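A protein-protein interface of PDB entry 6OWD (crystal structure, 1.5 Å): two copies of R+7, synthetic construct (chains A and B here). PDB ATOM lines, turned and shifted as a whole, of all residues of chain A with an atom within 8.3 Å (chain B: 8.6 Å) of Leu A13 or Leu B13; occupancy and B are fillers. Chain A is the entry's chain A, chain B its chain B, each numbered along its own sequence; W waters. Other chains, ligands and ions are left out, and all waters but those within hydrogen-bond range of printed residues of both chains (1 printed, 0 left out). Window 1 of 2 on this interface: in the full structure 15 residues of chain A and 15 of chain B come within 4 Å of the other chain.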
ATOM      1  N   LEU A   6     -26.462   3.439  -4.262  1.00  0.00           N
ATOM      2  CA  LEU A   6     -26.896   2.987  -5.590  1.00  0.00           C
ATOM      3  C   LEU A   6     -27.910   3.944  -6.213  1.00  0.00           C
ATOM      4  O   LEU A   6     -27.882   4.203  -7.415  1.00  0.00           O
ATOM      5  CB  LEU A   6     -27.434   1.560  -5.496  1.00  0.00           C
ATOM      6  CG  LEU A   6     -26.448   0.505  -5.019  1.00  0.00           C
ATOM      7  CD1 LEU A   6     -27.222  -0.807  -4.800  1.00  0.00           C
ATOM      8  CD2 LEU A   6     -25.370   0.315  -5.901  1.00  0.00           C
ATOM      9  N   GLN A   7     -28.888   4.385  -5.452  1.00  0.00           N
ATOM     10  CA  GLN A   7     -29.825   5.347  -6.005  1.00  0.00           C
ATOM     11  C   GLN A   7     -29.151   6.628  -6.431  1.00  0.00           C
ATOM     12  O   GLN A   7     -29.456   7.141  -7.522  1.00  0.00           O
ATOM     13  CB  GLN A   7     -30.916   5.576  -4.976  1.00  0.00           C
ATOM     14  CG  GLN A   7     -31.943   4.430  -4.863  1.00  0.00           C
ATOM     15  CD  GLN A   7     -32.977   4.564  -3.745  1.00  0.00           C
ATOM     16  OE1 GLN A   7     -33.035   5.531  -3.017  1.00  0.00           O
ATOM     17  NE2 GLN A   7     -33.805   3.553  -3.609  1.00  0.00           N
ATOM     18  N   ARG A   8     -28.229   7.165  -5.618  1.00  0.00           N
ATOM     19  CA  ARG A   8     -27.482   8.350  -6.066  1.00  0.00           C
ATOM     20  C   ARG A   8     -26.680   8.071  -7.331  1.00  0.00           C
ATOM     21  O   ARG A   8     -26.586   8.928  -8.209  1.00  0.00           O
ATOM     22  CB  ARG A   8     -26.560   8.847  -4.984  1.00  0.00           C
ATOM     23  CG  ARG A   8     -27.310   9.590  -3.960  1.00  0.00           C
ATOM     24  CD  ARG A   8     -26.291  10.256  -2.942  1.00  0.00           C
ATOM     25  NE  ARG A   8     -25.367   9.299  -2.281  1.00  0.00           N
ATOM     26  CZ  ARG A   8     -25.561   8.741  -1.083  1.00  0.00           C
ATOM     27  NH1 ARG A   8     -26.594   9.098  -0.362  1.00  0.00           N
ATOM     28  NH2 ARG A   8     -24.669   7.887  -0.603  1.00  0.00           N
ATOM     29  N   GLN A   9     -26.079   6.886  -7.433  1.00  0.00           N
ATOM     30  CA  GLN A   9     -25.283   6.566  -8.609  1.00  0.00           C
ATOM     31  C   GLN A   9     -26.157   6.492  -9.865  1.00  0.00           C
ATOM     32  O   GLN A   9     -25.768   6.958 -10.950  1.00  0.00           O
ATOM     33  CB  GLN A   9     -24.533   5.272  -8.325  1.00  0.00           C
ATOM     34  CG  GLN A   9     -23.690   4.862  -9.520  1.00  0.00           C
ATOM     35  CD  GLN A   9     -22.813   3.633  -9.258  1.00  0.00           C
ATOM     36  OE1 GLN A   9     -22.944   2.966  -8.217  1.00  0.00           O
ATOM     37  NE2 GLN A   9     -21.878   3.348 -10.207  1.00  0.00           N
ATOM     38  N   ILE A  10     -27.384   5.999  -9.716  1.00  0.00           N
ATOM     39  CA  ILE A  10     -28.268   5.936 -10.870  1.00  0.00           C
ATOM     40  C   ILE A  10     -28.604   7.323 -11.337  1.00  0.00           C
ATOM     41  O   ILE A  10     -28.576   7.601 -12.545  1.00  0.00           O
ATOM     42  CB  ILE A  10     -29.535   5.158 -10.533  1.00  0.00           C
ATOM     43  CG1 ILE A  10     -29.225   3.701 -10.397  1.00  0.00           C
ATOM     44  CG2 ILE A  10     -30.628   5.325 -11.543  1.00  0.00           C
ATOM     45  CD1 ILE A  10     -30.365   2.888  -9.599  1.00  0.00           C
ATOM     46  N   ARG A  11     -28.938   8.212 -10.389  1.00  0.00           N
ATOM     47  CA  ARG A  11     -29.312   9.563 -10.787  1.00  0.00           C
ATOM     48  C   ARG A  11     -28.127  10.291 -11.434  1.00  0.00           C
ATOM     49  O   ARG A  11     -28.306  10.945 -12.460  1.00  0.00           O
ATOM     50  CB  ARG A  11     -29.888  10.308  -9.590  1.00  0.00           C
ATOM     51  CG  ARG A  11     -31.184   9.802  -9.061  1.00  0.00           C
ATOM     52  CD  ARG A  11     -32.337   9.880 -10.045  1.00  0.00           C
ATOM     53  NE  ARG A  11     -33.595   9.388  -9.433  1.00  0.00           N
ATOM     54  CZ  ARG A  11     -34.418   8.497  -9.987  1.00  0.00           C
ATOM     55  NH1 ARG A  11     -34.153   8.029 -11.187  1.00  0.00           N
ATOM     56  NH2 ARG A  11     -35.514   8.079  -9.345  1.00  0.00           N
ATOM     57  N   ALA A  12     -26.905  10.052 -10.959  1.00  0.00           N
ATOM     58  CA  ALA A  12     -25.702  10.622 -11.564  1.00  0.00           C
ATOM     59  C   ALA A  12     -25.493  10.106 -12.977  1.00  0.00           C
ATOM     60  O   ALA A  12     -25.226  10.876 -13.889  1.00  0.00           O
ATOM     61  CB  ALA A  12     -24.525  10.284 -10.669  1.00  0.00           C
ATOM     62  N   LEU A  13     -25.714   8.819 -13.185  1.00  0.00           N
ATOM     63  CA  LEU A  13     -25.554   8.200 -14.486  1.00  0.00           C
ATOM     64  C   LEU A  13     -26.600   8.695 -15.455  1.00  0.00           C
ATOM     65  O   LEU A  13     -26.375   8.784 -16.657  1.00  0.00           O
ATOM     66  CB  LEU A  13     -25.639   6.692 -14.298  1.00  0.00           C
ATOM     67  CG  LEU A  13     -24.372   5.952 -13.818  1.00  0.00           C
ATOM     68  CD1 LEU A  13     -24.735   4.416 -13.548  1.00  0.00           C
ATOM     69  CD2 LEU A  13     -23.266   6.068 -14.805  1.00  0.00           C
ATOM     70  N   GLN A  14     -27.800   8.890 -14.962  1.00  0.00           N
ATOM     71  CA  GLN A  14     -28.843   9.456 -15.802  1.00  0.00           C
ATOM     72  C   GLN A  14     -28.527  10.891 -16.221  1.00  0.00           C
ATOM     73  O   GLN A  14     -28.828  11.271 -17.354  1.00  0.00           O
ATOM     74  CB  GLN A  14     -30.206   9.352 -15.068  1.00  0.00           C
ATOM     75  CG  GLN A  14     -30.717   7.946 -14.928  1.00  0.00           C
ATOM     76  CD  GLN A  14     -31.957   7.809 -14.092  1.00  0.00           C
ATOM     77  OE1 GLN A  14     -32.187   8.561 -13.161  1.00  0.00           O
ATOM     78  NE2 GLN A  14     -32.723   6.767 -14.369  1.00  0.00           N
ATOM     79  N   ARG A  15     -28.004  11.708 -15.303  1.00  0.00           N
ATOM     80  CA  ARG A  15     -27.545  13.052 -15.643  1.00  0.00           C
ATOM     81  C   ARG A  15     -26.419  12.985 -16.669  1.00  0.00           C
ATOM     82  O   ARG A  15     -26.422  13.714 -17.649  1.00  0.00           O
ATOM     83  CB  ARG A  15     -27.109  13.760 -14.361  1.00  0.00           C
ATOM     84  CG  ARG A  15     -26.984  15.258 -14.514  1.00  0.00           C
ATOM     85  CD  ARG A  15     -26.643  15.919 -13.154  1.00  0.00           C
ATOM     86  NE  ARG A  15     -27.833  16.045 -12.319  1.00  0.00           N
ATOM     87  CZ  ARG A  15     -27.978  16.953 -11.348  1.00  0.00           C
ATOM     88  NH1 ARG A  15     -26.973  17.797 -11.087  1.00  0.00           N
ATOM     89  NH2 ARG A  15     -29.120  17.027 -10.636  1.00  0.00           N
ATOM     90  N   GLN A  16     -25.465  12.075 -16.485  1.00  0.00           N
ATOM     91  CA  GLN A  16     -24.412  11.927 -17.484  1.00  0.00           C
ATOM     92  C   GLN A  16     -24.982  11.535 -18.843  1.00  0.00           C
ATOM     93  O   GLN A  16     -24.575  12.069 -19.866  1.00  0.00           O
ATOM     94  CB  GLN A  16     -23.416  10.895 -16.977  1.00  0.00           C
ATOM     95  CG  GLN A  16     -22.297  10.549 -17.907  1.00  0.00           C
ATOM     96  CD  GLN A  16     -21.383  11.742 -18.230  1.00  0.00           C
ATOM     97  OE1 GLN A  16     -21.633  12.861 -17.800  1.00  0.00           O
ATOM     98  NE2 GLN A  16     -20.307  11.484 -19.015  1.00  0.00           N
ATOM     99  N   ASN A  17     -25.917  10.575 -18.861  1.00  0.00           N
ATOM    100  CA  ASN A  17     -26.589  10.171 -20.084  1.00  0.00           C
ATOM    101  C   ASN A  17     -27.131  11.379 -20.824  1.00  0.00           C
ATOM    102  O   ASN A  17     -27.029  11.468 -22.040  1.00  0.00           O
ATOM    103  CB  ASN A  17     -27.699   9.174 -19.717  1.00  0.00           C
ATOM    104  CG  ASN A  17     -28.392   8.576 -20.958  1.00  0.00           C
ATOM    105  OD1 ASN A  17     -29.359   9.114 -21.485  1.00  0.00           O
ATOM    106  ND2 ASN A  17     -27.826   7.518 -21.470  1.00  0.00           N
ATOM    107  N   ALA A  18     -27.831  12.243 -20.116  1.00  0.00           N
ATOM    108  CA  ALA A  18     -28.391  13.405 -20.783  1.00  0.00           C
ATOM    109  C   ALA A  18     -27.296  14.301 -21.310  1.00  0.00           C
ATOM    110  O   ALA A  18     -27.426  14.848 -22.401  1.00  0.00           O
ATOM    111  CB  ALA A  18     -29.268  14.163 -19.817  1.00  0.00           C
ATOM    112  N   ARG A  19     -26.222  14.502 -20.533  1.00  0.00           N
ATOM    113  CA  ARG A  19     -25.132  15.342 -21.020  1.00  0.00           C
ATOM    114  C   ARG A  19     -24.484  14.776 -22.283  1.00  0.00           C
ATOM    115  O   ARG A  19     -24.062  15.519 -23.158  1.00  0.00           O
ATOM    116  CB  ARG A  19     -24.084  15.505 -19.923  1.00  0.00           C
ATOM    117  CG  ARG A  19     -24.479  16.609 -18.881  1.00  0.00           C
ATOM    118  CD  ARG A  19     -23.621  16.494 -17.619  1.00  0.00           C
ATOM    119  NE  ARG A  19     -23.963  17.575 -16.693  1.00  0.00           N
ATOM    120  CZ  ARG A  19     -23.589  17.633 -15.419  1.00  0.00           C
ATOM    121  NH1 ARG A  19     -22.885  16.634 -14.913  1.00  0.00           N
ATOM    122  NH2 ARG A  19     -23.920  18.684 -14.654  1.00  0.00           N
ATOM    123  N   LEU A  20     -24.332  13.471 -22.353  1.00  0.00           N
ATOM    124  CA  LEU A  20     -23.800  12.839 -23.551  1.00  0.00           C
ATOM    125  C   LEU A  20     -24.738  13.005 -24.737  1.00  0.00           C
ATOM    126  O   LEU A  20     -24.268  13.212 -25.853  1.00  0.00           O
ATOM    127  CB  LEU A  20     -23.467  11.355 -23.236  1.00  0.00           C
ATOM    128  CG  LEU A  20     -22.431  11.230 -22.095  1.00  0.00           C
ATOM    129  CD1 LEU A  20     -22.206   9.787 -21.782  1.00  0.00           C
ATOM    130  CD2 LEU A  20     -21.104  11.913 -22.445  1.00  0.00           C
ATOM    131  N   LEU B   6     -31.344  -2.382  -8.412  1.00  0.00           N
ATOM    132  CA  LEU B   6     -30.576  -1.178  -8.551  1.00  0.00           C
ATOM    133  C   LEU B   6     -29.329  -1.480  -9.291  1.00  0.00           C
ATOM    134  O   LEU B   6     -28.891  -0.668 -10.098  1.00  0.00           O
ATOM    135  CB  LEU B   6     -30.260  -0.610  -7.186  1.00  0.00           C
ATOM    136  CG  LEU B   6     -31.521  -0.006  -6.555  1.00  0.00           C
ATOM    137  CD1 LEU B   6     -31.231   0.358  -5.025  1.00  0.00           C
ATOM    138  CD2 LEU B   6     -32.052   1.176  -7.171  1.00  0.00           C
ATOM    139  N   GLN B   7     -28.665  -2.562  -8.920  1.00  0.00           N
ATOM    140  CA  GLN B   7     -27.381  -2.896  -9.538  1.00  0.00           C
ATOM    141  C   GLN B   7     -27.542  -3.185 -11.022  1.00  0.00           C
ATOM    142  O   GLN B   7     -26.719  -2.719 -11.847  1.00  0.00           O
ATOM    143  CB  GLN B   7     -26.721  -4.071  -8.831  1.00  0.00           C
ATOM    144  CG  GLN B   7     -26.181  -3.798  -7.452  1.00  0.00           C
ATOM    145  CD  GLN B   7     -25.733  -5.084  -6.762  1.00  0.00           C
ATOM    146  OE1 GLN B   7     -25.983  -6.187  -7.263  1.00  0.00           O
ATOM    147  NE2 GLN B   7     -25.135  -4.957  -5.596  1.00  0.00           N
ATOM    148  N   ARG B   8     -28.674  -3.803 -11.407  1.00  0.00           N
ATOM    149  CA  ARG B   8     -28.907  -4.073 -12.833  1.00  0.00           C
ATOM    150  C   ARG B   8     -29.161  -2.779 -13.595  1.00  0.00           C
ATOM    151  O   ARG B   8     -28.720  -2.649 -14.739  1.00  0.00           O
ATOM    152  CB  ARG B   8     -30.065  -5.050 -13.026  1.00  0.00           C
ATOM    153  CG  ARG B   8     -29.686  -6.452 -12.637  1.00  0.00           C
ATOM    154  CD  ARG B   8     -30.699  -7.459 -13.083  1.00  0.00           C
ATOM    155  NE  ARG B   8     -31.959  -7.379 -12.355  1.00  0.00           N
ATOM    156  CZ  ARG B   8     -32.168  -7.984 -11.204  1.00  0.00           C
ATOM    157  NH1 ARG B   8     -31.186  -8.668 -10.626  1.00  0.00           N
ATOM    158  NH2 ARG B   8     -33.320  -7.870 -10.620  1.00  0.00           N
ATOM    159  N   GLN B   9     -29.841  -1.810 -12.968  1.00  0.00           N
ATOM    160  CA  GLN B   9     -30.127  -0.523 -13.592  1.00  0.00           C
ATOM    161  C   GLN B   9     -28.850   0.276 -13.781  1.00  0.00           C
ATOM    162  O   GLN B   9     -28.665   0.929 -14.818  1.00  0.00           O
ATOM    163  CB  GLN B   9     -31.114   0.261 -12.740  1.00  0.00           C
ATOM    164  CG  GLN B   9     -31.572   1.560 -13.385  1.00  0.00           C
ATOM    165  CD  GLN B   9     -32.691   2.232 -12.636  1.00  0.00           C
ATOM    166  OE1 GLN B   9     -33.079   1.813 -11.525  1.00  0.00           O
ATOM    167  NE2 GLN B   9     -33.253   3.270 -13.262  1.00  0.00           N
ATOM    168  N   ILE B  10     -27.952   0.200 -12.797  1.00  0.00           N
ATOM    169  CA  ILE B  10     -26.647   0.824 -12.982  1.00  0.00           C
ATOM    170  C   ILE B  10     -25.916   0.201 -14.162  1.00  0.00           C
ATOM    171  O   ILE B  10     -25.323   0.918 -14.975  1.00  0.00           O
ATOM    172  CB  ILE B  10     -25.851   0.728 -11.688  1.00  0.00           C
ATOM    173  CG1 ILE B  10     -26.483   1.650 -10.675  1.00  0.00           C
ATOM    174  CG2 ILE B  10     -24.425   1.065 -11.938  1.00  0.00           C
ATOM    175  CD1 ILE B  10     -26.124   1.186  -9.273  1.00  0.00           C
ATOM    176  N   ARG B  11     -25.882  -1.155 -14.249  1.00  0.00           N
ATOM    177  CA  ARG B  11     -25.140  -1.776 -15.351  1.00  0.00           C
ATOM    178  C   ARG B  11     -25.739  -1.395 -16.701  1.00  0.00           C
ATOM    179  O   ARG B  11     -25.003  -1.079 -17.636  1.00  0.00           O
ATOM    180  CB  ARG B  11     -25.108  -3.293 -15.173  1.00  0.00           C
ATOM    181  CG  ARG B  11     -24.258  -3.714 -14.073  1.00  0.00           C
ATOM    182  CD  ARG B  11     -22.781  -3.682 -14.400  1.00  0.00           C
ATOM    183  NE  ARG B  11     -21.969  -4.151 -13.258  1.00  0.00           N
ATOM    184  CZ  ARG B  11     -21.460  -3.355 -12.307  1.00  0.00           C
ATOM    185  NH1 ARG B  11     -21.655  -2.043 -12.359  1.00  0.00           N
ATOM    186  NH2 ARG B  11     -20.722  -3.862 -11.304  1.00  0.00           N
ATOM    187  N   ALA B  12     -27.053  -1.300 -16.801  1.00  0.00           N
ATOM    188  CA  ALA B  12     -27.665  -0.894 -18.067  1.00  0.00           C
ATOM    189  C   ALA B  12     -27.302   0.548 -18.447  1.00  0.00           C
ATOM    190  O   ALA B  12     -26.897   0.808 -19.572  1.00  0.00           O
ATOM    191  CB  ALA B  12     -29.181  -1.078 -17.989  1.00  0.00           C
ATOM    192  N   LEU B  13     -27.346   1.472 -17.478  1.00  0.00           N
ATOM    193  CA  LEU B  13     -26.950   2.849 -17.723  1.00  0.00           C
ATOM    194  C   LEU B  13     -25.493   2.940 -18.092  1.00  0.00           C
ATOM    195  O   LEU B  13     -25.128   3.768 -18.922  1.00  0.00           O
ATOM    196  CB  LEU B  13     -27.243   3.679 -16.502  1.00  0.00           C
ATOM    197  CG  LEU B  13     -28.753   4.071 -16.412  1.00  0.00           C
ATOM    198  CD1 LEU B  13     -29.044   4.450 -14.977  1.00  0.00           C
ATOM    199  CD2 LEU B  13     -29.055   5.188 -17.354  1.00  0.00           C
ATOM    200  N   GLN B  14     -24.652   2.133 -17.470  1.00  0.00           N
ATOM    201  CA  GLN B  14     -23.240   2.148 -17.804  1.00  0.00           C
ATOM    202  C   GLN B  14     -23.009   1.676 -19.232  1.00  0.00           C
ATOM    203  O   GLN B  14     -22.187   2.253 -19.955  1.00  0.00           O
ATOM    204  CB  GLN B  14     -22.494   1.287 -16.814  1.00  0.00           C
ATOM    205  CG  GLN B  14     -22.232   1.985 -15.493  1.00  0.00           C
ATOM    206  CD  GLN B  14     -21.725   1.052 -14.390  1.00  0.00           C
ATOM    207  OE1 GLN B  14     -21.930  -0.165 -14.385  1.00  0.00           O
ATOM    208  NE2 GLN B  14     -21.188   1.660 -13.364  1.00  0.00           N
ATOM    209  N   ARG B  15     -23.721   0.636 -19.646  1.00  0.00           N
ATOM    210  CA  ARG B  15     -23.693   0.175 -21.041  1.00  0.00           C
ATOM    211  C   ARG B  15     -24.180   1.256 -22.003  1.00  0.00           C
ATOM    212  O   ARG B  15     -23.566   1.494 -23.040  1.00  0.00           O
ATOM    213  CB  ARG B  15     -24.576  -1.050 -21.228  1.00  0.00           C
ATOM    214  CG  ARG B  15     -24.049  -2.309 -20.721  1.00  0.00           C
ATOM    215  CD  ARG B  15     -25.112  -3.440 -20.785  1.00  0.00           C
ATOM    216  NE  ARG B  15     -25.103  -4.300 -19.584  1.00  0.00           N
ATOM    217  CZ  ARG B  15     -24.021  -4.919 -19.092  1.00  0.00           C
ATOM    218  NH1 ARG B  15     -22.830  -4.790 -19.682  1.00  0.00           N
ATOM    219  NH2 ARG B  15     -24.124  -5.671 -18.004  1.00  0.00           N
ATOM    220  N   GLN B  16     -25.286   1.905 -21.669  1.00  0.00           N
ATOM    221  CA  GLN B  16     -25.822   2.952 -22.525  1.00  0.00           C
ATOM    222  C   GLN B  16     -24.836   4.085 -22.661  1.00  0.00           C
ATOM    223  O   GLN B  16     -24.605   4.594 -23.755  1.00  0.00           O
ATOM    224  CB  GLN B  16     -27.122   3.469 -21.938  1.00  0.00           C
ATOM    225  CG  GLN B  16     -28.274   2.434 -21.994  1.00  0.00           C
ATOM    226  CD  GLN B  16     -29.529   2.941 -21.285  1.00  0.00           C
ATOM    227  OE1 GLN B  16     -29.865   4.135 -21.354  1.00  0.00           O
ATOM    228  NE2 GLN B  16     -30.201   2.052 -20.567  1.00  0.00           N
ATOM    229  N   ASN B  17     -24.297   4.531 -21.544  1.00  0.00           N
ATOM    230  CA  ASN B  17     -23.376   5.652 -21.601  1.00  0.00           C
ATOM    231  C   ASN B  17     -22.077   5.318 -22.351  1.00  0.00           C
ATOM    232  O   ASN B  17     -21.523   6.212 -23.026  1.00  0.00           O
ATOM    233  CB  ASN B  17     -23.063   6.135 -20.177  1.00  0.00           C
ATOM    234  CG  ASN B  17     -24.201   6.842 -19.510  1.00  0.00           C
ATOM    235  OD1 ASN B  17     -25.252   7.110 -20.098  1.00  0.00           O
ATOM    236  ND2 ASN B  17     -23.978   7.184 -18.229  1.00  0.00           N
ATOM    237  N   ALA B  18     -21.557   4.104 -22.216  1.00  0.00           N
ATOM    238  CA  ALA B  18     -20.340   3.723 -22.960  1.00  0.00           C
ATOM    239  C   ALA B  18     -20.587   3.749 -24.457  1.00  0.00           C
ATOM    240  O   ALA B  18     -19.762   4.271 -25.217  1.00  0.00           O
ATOM    241  CB  ALA B  18     -19.870   2.351 -22.520  1.00  0.00           C
ATOM    242  N   ARG B  19     -21.795   3.350 -24.871  1.00  0.00           N
ATOM    243  CA  ARG B  19     -22.218   3.428 -26.268  1.00  0.00           C
ATOM    244  C   ARG B  19     -22.273   4.849 -26.766  1.00  0.00           C
ATOM    245  O   ARG B  19     -21.701   5.173 -27.806  1.00  0.00           O
ATOM    246  CB  ARG B  19     -23.583   2.820 -26.387  1.00  0.00           C
ATOM    247  CG  ARG B  19     -24.011   2.377 -27.718  1.00  0.00           C
ATOM    248  CD  ARG B  19     -25.360   1.618 -27.620  1.00  0.00           C
ATOM    249  NE  ARG B  19     -25.957   1.410 -28.931  1.00  0.00           N
ATOM    250  CZ  ARG B  19     -25.532   0.511 -29.782  1.00  0.00           C
ATOM    251  NH1 ARG B  19     -24.520  -0.277 -29.459  1.00  0.00           N
ATOM    252  NH2 ARG B  19     -26.150   0.365 -30.926  1.00  0.00           N
ATOM    253  N   LEU B  20     -22.857   5.741 -25.975  1.00  0.00           N
ATOM    254  CA  LEU B  20     -22.853   7.122 -26.382  1.00  0.00           C
ATOM    255  C   LEU B  20     -21.438   7.687 -26.443  1.00  0.00           C
ATOM    256  O   LEU B  20     -21.145   8.481 -27.338  1.00  0.00           O
ATOM    257  CB  LEU B  20     -23.708   7.899 -25.417  1.00  0.00           C
ATOM    258  CG  LEU B  20     -25.200   7.697 -25.538  1.00  0.00           C
ATOM    259  CD1 LEU B  20     -25.934   8.444 -24.355  1.00  0.00           C
ATOM    260  CD2 LEU B  20     -25.773   8.126 -26.787  1.00  0.00           C
HETATM  261  O   HOH W   1     -32.629   4.087 -16.197  1.00  0.00           O
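Leu A6 touches Ile B10, and with the chains exchanged Ile A10 touches Leu B6. Gln A9 touches Ile B10, and with the chains exchanged Ile A10 touches Gln B9. Ile A10 touches its own counterpart, Ile B10. Ile A10 touches Leu B13, and with the chains exchanged Leu A13 touches Ile B10. Positions printed for both chains: 6, 7, 8, 9, 10, 11, 12, 13, 14, 15, 16, 17, 18, 19 and 20.
O of Leu A13 is in hydrogen-bond range of ND2 of Asn B17. ND2 of Asn A17 is in hydrogen-bond range of OD1 of Asn B17.
Hydrophobic or aromatic side chains of chain A that line the printed part of chain B: Leu A6, Ile A10, Leu A13 and Leu A20. Hydrophobic or aromatic side chains of chain B within 4 Å of the printed part of chain A: Leu B6, Ile B10, Leu B13 and Leu B20. Among the printed residues, 21 pairs touch across the chains. Among the printed residues, no Asp or Glu carboxylate lies within 4 Å of a Lys or Arg side-chain nitrogen of the other chain.
The guanidinium group of Arg A11 is in hydrogen-bond range of the side-chain amide oxygen of Gln A14 (2.8 Å). The guanidinium group of Arg B11 lies within hydrogen-bond range of the side-chain amide oxygen of Gln B14 (2.8 Å).
Water W1 bridges NE2 of Gln B9 and NE2 of Gln A14.
Leu A6 touches Ile B10 (CD2 to CD1, 3.6 Å). Gln A7 touches Leu B6. OE1 of Gln A9 touches CD1 of Ile B10, 3.8 Å away. NE2 of Gln A9 touches NE2 of Gln B14, 3.6 Å away. CD2 of Leu B6 touches CD1 of Ile A10, 3.4 Å away. Ile A10 touches Leu B13 (CG2 to CD1, 3.9 Å). Leu A13 touches Ile B10 (CD1 to CG2, 3.7 Å). Leu A13 touches Gln B14 (CD1 to CG, 3.99 Å). Gln B9 touches Gln A14 (NE2 to NE2, 3.7 Å). CD1 of Leu A20 touches O of Asn B17, at 3.8 Å.
Printed residues of chain B within 4 Å of Gln A9: Ile B10 and Gln B14. No residue of chain B comes within 4 Å of Ala A12. Printed residues of chain B within 4 Å of Leu A13: Ile B10, Leu B13, Gln B14 and Asn B17. Of the printed residues of chain A, Ile B10 touches Leu A6 (3.6 Å), Gln A9 (3.8 Å), Ile A10 (3.4 Å) and Leu A13 (3.7 Å). No residue of chain A comes within 4 Å of Ala B12. Leu B13 touches three residues of chain A. Of the printed residues of chain A, Gln B14 touches Gln A9 and Leu A13. Arg B15 touches none of the printed residues of chain A.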
